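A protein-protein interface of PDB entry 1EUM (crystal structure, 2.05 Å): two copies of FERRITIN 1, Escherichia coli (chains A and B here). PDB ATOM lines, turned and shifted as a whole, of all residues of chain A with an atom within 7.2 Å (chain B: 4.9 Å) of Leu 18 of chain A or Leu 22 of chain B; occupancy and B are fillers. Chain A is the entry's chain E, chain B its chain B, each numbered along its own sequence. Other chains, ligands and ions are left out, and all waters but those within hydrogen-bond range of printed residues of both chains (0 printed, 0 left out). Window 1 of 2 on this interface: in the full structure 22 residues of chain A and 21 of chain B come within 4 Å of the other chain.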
ATOM      1  N   GLU A  12     -12.925  10.980 -20.406  1.00  0.00           N
ATOM      2  CA  GLU A  12     -12.626  10.218 -19.216  1.00  0.00           C
ATOM      3  C   GLU A  12     -11.487  10.859 -18.440  1.00  0.00           C
ATOM      4  O   GLU A  12     -11.533  10.937 -17.219  1.00  0.00           O
ATOM      5  CB  GLU A  12     -12.266   8.786 -19.576  1.00  0.00           C
ATOM      6  CG  GLU A  12     -13.442   7.847 -19.583  1.00  0.00           C
ATOM      7  CD  GLU A  12     -13.155   6.581 -20.361  1.00  0.00           C
ATOM      8  OE1 GLU A  12     -14.106   6.010 -20.952  1.00  0.00           O
ATOM      9  OE2 GLU A  12     -11.973   6.160 -20.388  1.00  0.00           O
ATOM     10  N   GLN A  13     -10.468  11.330 -19.151  1.00  0.00           N
ATOM     11  CA  GLN A  13      -9.330  11.957 -18.493  1.00  0.00           C
ATOM     12  C   GLN A  13      -9.757  13.208 -17.784  1.00  0.00           C
ATOM     13  O   GLN A  13      -9.292  13.494 -16.683  1.00  0.00           O
ATOM     14  CB  GLN A  13      -8.220  12.292 -19.486  1.00  0.00           C
ATOM     15  CG  GLN A  13      -6.959  12.847 -18.821  1.00  0.00           C
ATOM     16  CD  GLN A  13      -6.332  11.856 -17.859  1.00  0.00           C
ATOM     17  OE1 GLN A  13      -6.389  10.647 -18.070  1.00  0.00           O
ATOM     18  NE2 GLN A  13      -5.747  12.366 -16.785  1.00  0.00           N
ATOM     19  N   MET A  14     -10.636  13.969 -18.422  1.00  0.00           N
ATOM     20  CA  MET A  14     -11.143  15.202 -17.831  1.00  0.00           C
ATOM     21  C   MET A  14     -11.862  14.891 -16.512  1.00  0.00           C
ATOM     22  O   MET A  14     -11.697  15.590 -15.522  1.00  0.00           O
ATOM     23  CB  MET A  14     -12.093  15.921 -18.799  1.00  0.00           C
ATOM     24  CG  MET A  14     -12.813  17.129 -18.168  1.00  0.00           C
ATOM     25  SD  MET A  14     -14.167  17.718 -19.147  1.00  0.00           S
ATOM     26  CE  MET A  14     -15.370  16.483 -18.801  1.00  0.00           C
ATOM     27  N   ASN A  15     -12.628  13.812 -16.500  1.00  0.00           N
ATOM     28  CA  ASN A  15     -13.332  13.416 -15.297  1.00  0.00           C
ATOM     29  C   ASN A  15     -12.377  12.901 -14.234  1.00  0.00           C
ATOM     30  O   ASN A  15     -12.575  13.144 -13.049  1.00  0.00           O
ATOM     31  CB  ASN A  15     -14.407  12.396 -15.614  1.00  0.00           C
ATOM     32  CG  ASN A  15     -15.686  13.050 -16.102  1.00  0.00           C
ATOM     33  OD1 ASN A  15     -16.436  13.619 -15.317  1.00  0.00           O
ATOM     34  ND2 ASN A  15     -15.883  13.056 -17.412  1.00  0.00           N
ATOM     35  N   LEU A  16     -11.313  12.234 -14.660  1.00  0.00           N
ATOM     36  CA  LEU A  16     -10.316  11.745 -13.716  1.00  0.00           C
ATOM     37  C   LEU A  16      -9.594  12.937 -13.060  1.00  0.00           C
ATOM     38  O   LEU A  16      -9.308  12.932 -11.851  1.00  0.00           O
ATOM     39  CB  LEU A  16      -9.319  10.814 -14.408  1.00  0.00           C
ATOM     40  CG  LEU A  16      -8.143  10.405 -13.541  1.00  0.00           C
ATOM     41  CD1 LEU A  16      -8.646   9.660 -12.330  1.00  0.00           C
ATOM     42  CD2 LEU A  16      -7.144   9.569 -14.332  1.00  0.00           C
ATOM     43  N   GLU A  17      -9.313  13.968 -13.848  1.00  0.00           N
ATOM     44  CA  GLU A  17      -8.656  15.136 -13.302  1.00  0.00           C
ATOM     45  C   GLU A  17      -9.555  15.817 -12.262  1.00  0.00           C
ATOM     46  O   GLU A  17      -9.068  16.337 -11.256  1.00  0.00           O
ATOM     47  CB  GLU A  17      -8.296  16.124 -14.409  1.00  0.00           C
ATOM     48  CG  GLU A  17      -7.189  15.662 -15.336  1.00  0.00           C
ATOM     49  CD  GLU A  17      -5.825  15.653 -14.669  1.00  0.00           C
ATOM     50  OE1 GLU A  17      -5.702  16.148 -13.535  1.00  0.00           O
ATOM     51  OE2 GLU A  17      -4.875  15.164 -15.291  1.00  0.00           O
ATOM     52  N   LEU A  18     -10.863  15.831 -12.533  1.00  0.00           N
ATOM     53  CA  LEU A  18     -11.842  16.453 -11.639  1.00  0.00           C
ATOM     54  C   LEU A  18     -11.874  15.692 -10.327  1.00  0.00           C
ATOM     55  O   LEU A  18     -11.758  16.272  -9.250  1.00  0.00           O
ATOM     56  CB  LEU A  18     -13.237  16.465 -12.289  1.00  0.00           C
ATOM     57  CG  LEU A  18     -14.433  16.839 -11.395  1.00  0.00           C
ATOM     58  CD1 LEU A  18     -14.228  18.175 -10.726  1.00  0.00           C
ATOM     59  CD2 LEU A  18     -15.709  16.856 -12.187  1.00  0.00           C
ATOM     60  N   TYR A  19     -11.974  14.379 -10.419  1.00  0.00           N
ATOM     61  CA  TYR A  19     -11.966  13.563  -9.233  1.00  0.00           C
ATOM     62  C   TYR A  19     -10.656  13.762  -8.461  1.00  0.00           C
ATOM     63  O   TYR A  19     -10.650  13.843  -7.237  1.00  0.00           O
ATOM     64  CB  TYR A  19     -12.113  12.092  -9.604  1.00  0.00           C
ATOM     65  CG  TYR A  19     -11.880  11.185  -8.436  1.00  0.00           C
ATOM     66  CD1 TYR A  19     -10.650  10.556  -8.252  1.00  0.00           C
ATOM     67  CD2 TYR A  19     -12.852  11.027  -7.455  1.00  0.00           C
ATOM     68  CE1 TYR A  19     -10.418   9.763  -7.147  1.00  0.00           C
ATOM     69  CE2 TYR A  19     -12.637  10.220  -6.364  1.00  0.00           C
ATOM     70  CZ  TYR A  19     -11.424   9.593  -6.212  1.00  0.00           C
ATOM     71  OH  TYR A  19     -11.203   8.803  -5.118  1.00  0.00           O
ATOM     72  N   SER A  20      -9.546  13.817  -9.188  1.00  0.00           N
ATOM     73  CA  SER A  20      -8.238  13.960  -8.563  1.00  0.00           C
ATOM     74  C   SER A  20      -8.146  15.256  -7.770  1.00  0.00           C
ATOM     75  O   SER A  20      -7.581  15.298  -6.671  1.00  0.00           O
ATOM     76  CB  SER A  20      -7.146  13.901  -9.626  1.00  0.00           C
ATOM     77  OG  SER A  20      -7.172  12.644 -10.273  1.00  0.00           O
ATOM     78  N   SER A  21      -8.703  16.317  -8.331  1.00  0.00           N
ATOM     79  CA  SER A  21      -8.715  17.597  -7.651  1.00  0.00           C
ATOM     80  C   SER A  21      -9.493  17.509  -6.312  1.00  0.00           C
ATOM     81  O   SER A  21      -9.032  17.991  -5.277  1.00  0.00           O
ATOM     82  CB  SER A  21      -9.328  18.666  -8.554  1.00  0.00           C
ATOM     83  OG  SER A  21      -9.432  19.911  -7.875  1.00  0.00           O
ATOM     84  N   LEU A  22     -10.664  16.889  -6.343  1.00  0.00           N
ATOM     85  CA  LEU A  22     -11.471  16.770  -5.146  1.00  0.00           C
ATOM     86  C   LEU A  22     -10.793  15.851  -4.147  1.00  0.00           C
ATOM     87  O   LEU A  22     -10.890  16.050  -2.939  1.00  0.00           O
ATOM     88  CB  LEU A  22     -12.874  16.274  -5.493  1.00  0.00           C
ATOM     89  CG  LEU A  22     -13.589  17.196  -6.469  1.00  0.00           C
ATOM     90  CD1 LEU A  22     -14.971  16.693  -6.768  1.00  0.00           C
ATOM     91  CD2 LEU A  22     -13.634  18.586  -5.922  1.00  0.00           C
ATOM     92  N   LEU A  23     -10.080  14.858  -4.653  1.00  0.00           N
ATOM     93  CA  LEU A  23      -9.356  13.946  -3.789  1.00  0.00           C
ATOM     94  C   LEU A  23      -8.317  14.711  -2.974  1.00  0.00           C
ATOM     95  O   LEU A  23      -8.215  14.532  -1.767  1.00  0.00           O
ATOM     96  CB  LEU A  23      -8.681  12.842  -4.605  1.00  0.00           C
ATOM     97  CG  LEU A  23      -7.721  11.897  -3.855  1.00  0.00           C
ATOM     98  CD1 LEU A  23      -8.445  10.970  -2.870  1.00  0.00           C
ATOM     99  CD2 LEU A  23      -6.917  11.093  -4.829  1.00  0.00           C
ATOM    100  N   TYR A  24      -7.558  15.578  -3.631  1.00  0.00           N
ATOM    101  CA  TYR A  24      -6.536  16.360  -2.933  1.00  0.00           C
ATOM    102  C   TYR A  24      -7.158  17.343  -1.944  1.00  0.00           C
ATOM    103  O   TYR A  24      -6.618  17.588  -0.869  1.00  0.00           O
ATOM    104  CB  TYR A  24      -5.623  17.077  -3.931  1.00  0.00           C
ATOM    105  CG  TYR A  24      -4.848  16.112  -4.790  1.00  0.00           C
ATOM    106  CD1 TYR A  24      -4.632  14.811  -4.367  1.00  0.00           C
ATOM    107  CD2 TYR A  24      -4.342  16.494  -6.024  1.00  0.00           C
ATOM    108  CE1 TYR A  24      -3.928  13.909  -5.148  1.00  0.00           C
ATOM    109  CE2 TYR A  24      -3.642  15.600  -6.817  1.00  0.00           C
ATOM    110  CZ  TYR A  24      -3.445  14.307  -6.379  1.00  0.00           C
ATOM    111  OH  TYR A  24      -2.768  13.409  -7.175  1.00  0.00           O
ATOM    112  N   ALA A  47      -4.845  20.891  -5.245  1.00  0.00           N
ATOM    113  CA  ALA A  47      -6.191  20.627  -5.669  1.00  0.00           C
ATOM    114  C   ALA A  47      -6.525  21.658  -6.753  1.00  0.00           C
ATOM    115  O   ALA A  47      -7.158  21.341  -7.761  1.00  0.00           O
ATOM    116  CB  ALA A  47      -7.147  20.767  -4.488  1.00  0.00           C
ATOM    117  N   GLU A  50      -4.648  20.708 -10.072  1.00  0.00           N
ATOM    118  CA  GLU A  50      -5.277  19.629 -10.829  1.00  0.00           C
ATOM    119  C   GLU A  50      -6.556  20.092 -11.514  1.00  0.00           C
ATOM    120  O   GLU A  50      -6.935  19.567 -12.553  1.00  0.00           O
ATOM    121  CB  GLU A  50      -5.550  18.425  -9.933  1.00  0.00           C
ATOM    122  CG  GLU A  50      -5.339  17.094 -10.617  1.00  0.00           C
ATOM    123  CD  GLU A  50      -3.911  16.905 -11.072  1.00  0.00           C
ATOM    124  OE1 GLU A  50      -3.707  16.307 -12.145  1.00  0.00           O
ATOM    125  OE2 GLU A  50      -2.987  17.387 -10.372  1.00  0.00           O
ATOM    126  N   MET A  51      -7.212  21.083 -10.926  1.00  0.00           N
ATOM    127  CA  MET A  51      -8.438  21.625 -11.491  1.00  0.00           C
ATOM    128  C   MET A  51      -8.152  22.318 -12.819  1.00  0.00           C
ATOM    129  O   MET A  51      -8.967  22.270 -13.741  1.00  0.00           O
ATOM    130  CB  MET A  51      -9.101  22.600 -10.518  1.00  0.00           C
ATOM    131  CG  MET A  51     -10.548  22.928 -10.874  1.00  0.00           C
ATOM    132  SD  MET A  51     -11.661  21.475 -10.863  1.00  0.00           S
ATOM    133  CE  MET A  51     -12.894  22.019 -12.042  1.00  0.00           C
ATOM    134  N   HIS A  53      -5.779  21.426 -14.828  1.00  0.00           N
ATOM    135  CA  HIS A  53      -5.535  20.343 -15.769  1.00  0.00           C
ATOM    136  C   HIS A  53      -6.894  19.914 -16.314  1.00  0.00           C
ATOM    137  O   HIS A  53      -7.031  19.583 -17.494  1.00  0.00           O
ATOM    138  CB  HIS A  53      -4.842  19.144 -15.076  1.00  0.00           C
ATOM    139  CG  HIS A  53      -3.455  19.448 -14.590  1.00  0.00           C
ATOM    140  ND1 HIS A  53      -2.564  18.464 -14.220  1.00  0.00           N
ATOM    141  CD2 HIS A  53      -2.814  20.625 -14.404  1.00  0.00           C
ATOM    142  CE1 HIS A  53      -1.436  19.024 -13.819  1.00  0.00           C
ATOM    143  NE2 HIS A  53      -1.561  20.333 -13.927  1.00  0.00           N
ATOM    144  N   MET A  54      -7.906  19.942 -15.448  1.00  0.00           N
ATOM    145  CA  MET A  54      -9.261  19.570 -15.848  1.00  0.00           C
ATOM    146  C   MET A  54      -9.821  20.561 -16.866  1.00  0.00           C
ATOM    147  O   MET A  54     -10.319  20.175 -17.914  1.00  0.00           O
ATOM    148  CB  MET A  54     -10.185  19.493 -14.625  1.00  0.00           C
ATOM    149  CG  MET A  54     -11.601  19.027 -14.938  1.00  0.00           C
ATOM    150  SD  MET A  54     -12.750  20.398 -15.136  1.00  0.00           S
ATOM    151  CE  MET A  54     -14.261  19.622 -14.662  1.00  0.00           C
ATOM    152  N   PHE A  58     -11.179  20.325 -20.714  1.00  0.00           N
ATOM    153  CA  PHE A  58     -12.527  20.819 -20.919  1.00  0.00           C
ATOM    154  C   PHE A  58     -12.549  21.759 -22.128  1.00  0.00           C
ATOM    155  O   PHE A  58     -13.351  21.606 -23.036  1.00  0.00           O
ATOM    156  CB  PHE A  58     -12.963  21.580 -19.670  1.00  0.00           C
ATOM    157  CG  PHE A  58     -14.419  21.892 -19.632  1.00  0.00           C
ATOM    158  CD1 PHE A  58     -14.899  23.076 -20.156  1.00  0.00           C
ATOM    159  CD2 PHE A  58     -15.311  21.003 -19.071  1.00  0.00           C
ATOM    160  CE1 PHE A  58     -16.246  23.364 -20.138  1.00  0.00           C
ATOM    161  CE2 PHE A  58     -16.654  21.285 -19.041  1.00  0.00           C
ATOM    162  CZ  PHE A  58     -17.123  22.471 -19.582  1.00  0.00           C
ATOM    163  N   ILE A  70     -19.517  16.094 -17.767  1.00  0.00           N
ATOM    164  CA  ILE A  70     -19.115  15.813 -16.398  1.00  0.00           C
ATOM    165  C   ILE A  70     -20.026  14.721 -15.829  1.00  0.00           C
ATOM    166  O   ILE A  70     -21.255  14.861 -15.799  1.00  0.00           O
ATOM    167  CB  ILE A  70     -19.194  17.064 -15.523  1.00  0.00           C
ATOM    168  CG1 ILE A  70     -18.377  18.187 -16.147  1.00  0.00           C
ATOM    169  CG2 ILE A  70     -18.697  16.758 -14.113  1.00  0.00           C
ATOM    170  CD1 ILE A  70     -18.242  19.372 -15.254  1.00  0.00           C
ATOM    171  N   ASN A  71     -19.416  13.612 -15.444  1.00  0.00           N
ATOM    172  CA  ASN A  71     -20.137  12.478 -14.916  1.00  0.00           C
ATOM    173  C   ASN A  71     -20.185  12.508 -13.393  1.00  0.00           C
ATOM    174  O   ASN A  71     -19.591  13.377 -12.762  1.00  0.00           O
ATOM    175  CB  ASN A  71     -19.457  11.191 -15.367  1.00  0.00           C
ATOM    176  CG  ASN A  71     -19.501  11.015 -16.855  1.00  0.00           C
ATOM    177  OD1 ASN A  71     -20.486  11.370 -17.503  1.00  0.00           O
ATOM    178  ND2 ASN A  71     -18.428  10.477 -17.418  1.00  0.00           N
ATOM    179  N   THR A  72     -20.872  11.532 -12.814  1.00  0.00           N
ATOM    180  CA  THR A  72     -20.969  11.425 -11.369  1.00  0.00           C
ATOM    181  C   THR A  72     -19.573  11.274 -10.799  1.00  0.00           C
ATOM    182  O   THR A  72     -18.729  10.589 -11.375  1.00  0.00           O
ATOM    183  CB  THR A  72     -21.805  10.187 -10.945  1.00  0.00           C
ATOM    184  OG1 THR A  72     -23.169  10.373 -11.344  1.00  0.00           O
ATOM    185  CG2 THR A  72     -21.751  10.001  -9.422  1.00  0.00           C
ATOM    186  N   VAL A  73     -19.335  11.901  -9.658  1.00  0.00           N
ATOM    187  CA  VAL A  73     -18.048  11.802  -9.001  1.00  0.00           C
ATOM    188  C   VAL A  73     -18.202  11.019  -7.718  1.00  0.00           C
ATOM    189  O   VAL A  73     -18.986  11.388  -6.851  1.00  0.00           O
ATOM    190  CB  VAL A  73     -17.482  13.181  -8.621  1.00  0.00           C
ATOM    191  CG1 VAL A  73     -16.042  13.033  -8.129  1.00  0.00           C
ATOM    192  CG2 VAL A  73     -17.578  14.161  -9.780  1.00  0.00           C
ATOM    193  N   LEU B  18     -20.397  23.092  -4.331  1.00  0.00           N
ATOM    194  CA  LEU B  18     -19.523  22.307  -5.203  1.00  0.00           C
ATOM    195  C   LEU B  18     -20.311  21.857  -6.428  1.00  0.00           C
ATOM    196  O   LEU B  18     -19.869  22.028  -7.566  1.00  0.00           O
ATOM    197  CB  LEU B  18     -18.981  21.083  -4.458  1.00  0.00           C
ATOM    198  CG  LEU B  18     -18.288  20.011  -5.300  1.00  0.00           C
ATOM    199  CD1 LEU B  18     -17.185  20.622  -6.172  1.00  0.00           C
ATOM    200  CD2 LEU B  18     -17.737  18.917  -4.407  1.00  0.00           C
ATOM    201  N   TYR B  19     -21.484  21.283  -6.190  1.00  0.00           N
ATOM    202  CA  TYR B  19     -22.347  20.846  -7.277  1.00  0.00           C
ATOM    203  C   TYR B  19     -22.720  22.044  -8.169  1.00  0.00           C
ATOM    204  O   TYR B  19     -22.752  21.939  -9.385  1.00  0.00           O
ATOM    205  CB  TYR B  19     -23.635  20.209  -6.721  1.00  0.00           C
ATOM    206  CG  TYR B  19     -24.672  19.968  -7.795  1.00  0.00           C
ATOM    207  CD1 TYR B  19     -25.584  20.959  -8.150  1.00  0.00           C
ATOM    208  CD2 TYR B  19     -24.662  18.799  -8.529  1.00  0.00           C
ATOM    209  CE1 TYR B  19     -26.495  20.753  -9.168  1.00  0.00           C
ATOM    210  CE2 TYR B  19     -25.545  18.590  -9.552  1.00  0.00           C
ATOM    211  CZ  TYR B  19     -26.470  19.554  -9.863  1.00  0.00           C
ATOM    212  OH  TYR B  19     -27.358  19.309 -10.888  1.00  0.00           O
ATOM    213  N   SER B  20     -23.011  23.179  -7.548  1.00  0.00           N
ATOM    214  CA  SER B  20     -23.413  24.359  -8.289  1.00  0.00           C
ATOM    215  C   SER B  20     -22.313  24.852  -9.194  1.00  0.00           C
ATOM    216  O   SER B  20     -22.571  25.273 -10.313  1.00  0.00           O
ATOM    217  CB  SER B  20     -23.880  25.457  -7.341  1.00  0.00           C
ATOM    218  OG  SER B  20     -24.859  24.937  -6.459  1.00  0.00           O
ATOM    219  N   SER B  21     -21.075  24.772  -8.719  1.00  0.00           N
ATOM    220  CA  SER B  21     -19.942  25.176  -9.516  1.00  0.00           C
ATOM    221  C   SER B  21     -19.824  24.292 -10.798  1.00  0.00           C
ATOM    222  O   SER B  21     -19.608  24.799 -11.894  1.00  0.00           O
ATOM    223  CB  SER B  21     -18.665  25.087  -8.686  1.00  0.00           C
ATOM    224  OG  SER B  21     -17.520  25.259  -9.501  1.00  0.00           O
ATOM    225  N   LEU B  22     -19.995  22.984 -10.641  1.00  0.00           N
ATOM    226  CA  LEU B  22     -19.900  22.062 -11.769  1.00  0.00           C
ATOM    227  C   LEU B  22     -21.074  22.207 -12.720  1.00  0.00           C
ATOM    228  O   LEU B  22     -20.946  21.942 -13.914  1.00  0.00           O
ATOM    229  CB  LEU B  22     -19.776  20.617 -11.279  1.00  0.00           C
ATOM    230  CG  LEU B  22     -18.604  20.327 -10.320  1.00  0.00           C
ATOM    231  CD1 LEU B  22     -18.614  18.882  -9.908  1.00  0.00           C
ATOM    232  CD2 LEU B  22     -17.284  20.680 -10.948  1.00  0.00           C
ATOM    233  N   LEU B  23     -22.218  22.629 -12.189  1.00  0.00           N
ATOM    234  CA  LEU B  23     -23.413  22.827 -13.005  1.00  0.00           C
ATOM    235  C   LEU B  23     -23.217  23.978 -13.977  1.00  0.00           C
ATOM    236  O   LEU B  23     -23.578  23.878 -15.148  1.00  0.00           O
ATOM    237  CB  LEU B  23     -24.648  23.080 -12.125  1.00  0.00           C
ATOM    238  CG  LEU B  23     -25.922  23.561 -12.833  1.00  0.00           C
ATOM    239  CD1 LEU B  23     -26.491  22.478 -13.762  1.00  0.00           C
ATOM    240  CD2 LEU B  23     -26.958  23.994 -11.826  1.00  0.00           C
ATOM    241  N   TYR B  24     -22.639  25.079 -13.495  1.00  0.00           N
ATOM    242  CA  TYR B  24     -22.407  26.238 -14.359  1.00  0.00           C
ATOM    243  C   TYR B  24     -21.328  25.915 -15.386  1.00  0.00           C
ATOM    244  O   TYR B  24     -21.395  26.350 -16.530  1.00  0.00           O
ATOM    245  CB  TYR B  24     -22.041  27.476 -13.537  1.00  0.00           C
ATOM    246  CG  TYR B  24     -23.145  27.905 -12.596  1.00  0.00           C
ATOM    247  CD1 TYR B  24     -24.468  27.594 -12.865  1.00  0.00           C
ATOM    248  CD2 TYR B  24     -22.863  28.546 -11.401  1.00  0.00           C
ATOM    249  CE1 TYR B  24     -25.479  28.010 -12.043  1.00  0.00           C
ATOM    250  CE2 TYR B  24     -23.876  28.942 -10.548  1.00  0.00           C
ATOM    251  CZ  TYR B  24     -25.179  28.632 -10.854  1.00  0.00           C
ATOM    252  OH  TYR B  24     -26.189  28.983  -9.992  1.00  0.00           O
ATOM    253  N   GLN B  25     -20.348  25.118 -14.974  1.00  0.00           N
ATOM    254  CA  GLN B  25     -19.290  24.694 -15.876  1.00  0.00           C
ATOM    255  C   GLN B  25     -19.937  23.913 -17.018  1.00  0.00           C
ATOM    256  O   GLN B  25     -19.730  24.217 -18.187  1.00  0.00           O
ATOM    257  CB  GLN B  25     -18.293  23.804 -15.134  1.00  0.00           C
ATOM    258  CG  GLN B  25     -17.100  23.428 -15.955  1.00  0.00           C
ATOM    259  CD  GLN B  25     -15.979  24.402 -15.787  1.00  0.00           C
ATOM    260  OE1 GLN B  25     -15.405  24.513 -14.709  1.00  0.00           O
ATOM    261  NE2 GLN B  25     -15.685  25.161 -16.839  1.00  0.00           N
ATOM    262  N   GLN B  26     -20.752  22.924 -16.660  1.00  0.00           N
ATOM    263  CA  GLN B  26     -21.466  22.108 -17.640  1.00  0.00           C
ATOM    264  C   GLN B  26     -22.368  22.976 -18.515  1.00  0.00           C
ATOM    265  O   GLN B  26     -22.534  22.712 -19.694  1.00  0.00           O
ATOM    266  CB  GLN B  26     -22.298  21.038 -16.933  1.00  0.00           C
ATOM    267  CG  GLN B  26     -22.923  20.013 -17.861  1.00  0.00           C
ATOM    268  CD  GLN B  26     -21.885  19.175 -18.594  1.00  0.00           C
ATOM    269  OE1 GLN B  26     -21.779  19.236 -19.811  1.00  0.00           O
ATOM    270  NE2 GLN B  26     -21.141  18.381 -17.858  1.00  0.00           N
ATOM    271  N   MET B  51     -17.152  28.173  -6.676  1.00  0.00           N
ATOM    272  CA  MET B  51     -16.068  27.346  -6.131  1.00  0.00           C
ATOM    273  C   MET B  51     -15.535  28.061  -4.878  1.00  0.00           C
ATOM    274  O   MET B  51     -15.208  27.442  -3.863  1.00  0.00           O
ATOM    275  CB  MET B  51     -14.942  27.256  -7.157  1.00  0.00           C
ATOM    276  CG  MET B  51     -14.454  25.860  -7.496  1.00  0.00           C
ATOM    277  SD  MET B  51     -14.818  24.579  -6.307  1.00  0.00           S
ATOM    278  CE  MET B  51     -15.582  23.449  -7.336  1.00  0.00           C
ATOM    279  N   VAL B  73     -21.133  13.283  -5.997  1.00  0.00           N
ATOM    280  CA  VAL B  73     -21.671  14.405  -6.747  1.00  0.00           C
ATOM    281  C   VAL B  73     -22.422  13.876  -7.948  1.00  0.00           C
ATOM    282  O   VAL B  73     -21.885  13.088  -8.722  1.00  0.00           O
ATOM    283  CB  VAL B  73     -20.575  15.370  -7.241  1.00  0.00           C
ATOM    284  CG1 VAL B  73     -21.220  16.638  -7.799  1.00  0.00           C
ATOM    285  CG2 VAL B  73     -19.602  15.722  -6.110  1.00  0.00           C
ATOM    286  N   PRO B  76     -24.147  16.905 -13.465  1.00  0.00           N
ATOM    287  CA  PRO B  76     -24.951  18.104 -13.723  1.00  0.00           C
ATOM    288  C   PRO B  76     -25.402  18.156 -15.169  1.00  0.00           C
ATOM    289  O   PRO B  76     -26.029  19.122 -15.599  1.00  0.00           O
ATOM    290  CB  PRO B  76     -23.968  19.249 -13.456  1.00  0.00           C
ATOM    291  CG  PRO B  76     -22.642  18.670 -13.785  1.00  0.00           C
ATOM    292  CD  PRO B  76     -22.707  17.211 -13.390  1.00  0.00           C
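The side-chain amide nitrogen (NE2) of Gln 26 of chain B lies close to the backbone NH (N) of Ile 70 of chain A (2.8 Å).
The backbone carbonyl oxygen (O) of Val 73 of chain B lies within hydrogen-bond range of the backbone NH (N) of Val 73 of chain A, 3.0 Å away.
Among the printed residues, merely in contact across the chains: Leu 18 of chain A with Leu 22 of chain B, Phe 58 of chain A with Gln 25 of chain B, Ile 70 of chain A with Leu 22 of chain B, Ile 70 of chain A with Pro 76 of chain B and Thr 72 of chain A with Val 73 of chain B.
Leu 18 of chain A touches just one residue of chain B: Leu 22.
Of chain A, only Leu 18 (3.96 Å) and Ile 70 (3.96 Å) come within 4 Å of Leu 22 of chain B.
Of the printed residues of chain A, Gln 26 of chain B touches Ile 70 (2.8 Å).
Of the printed residues of chain B, Phe 58 of chain A touches Gln 25.
Of the printed residues of chain A, Val 73 of chain B touches Thr 72 and Val 73.
Printed residues of chain A within 4 Å of Gln 25 of chain B: Phe 58.
The nearest residue of chain A that does not touch Leu 22 of chain B is Met 51 of chain A (4.7 Å).
Printed residues of chain A that touch a printed residue of chain B: Leu 18, Phe 58, Ile 70, Thr 72 and Val 73.
Hydrophobic or aromatic side chains of chain A within 4 Å of the printed part of chain B: Leu 18, Phe 58 and Ile 70.
Leu 18 of chain A touches Leu 22 of chain B, but with the chains exchanged Leu 22 of chain A does not touch Leu 18 of chain B (4.1 Å).
Val 73 of chain A touches its own counterpart, Val 73 of chain B.
Positions printed for both chains: 18, 19, 20, 21, 22, 23, 24, 51 and 73.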
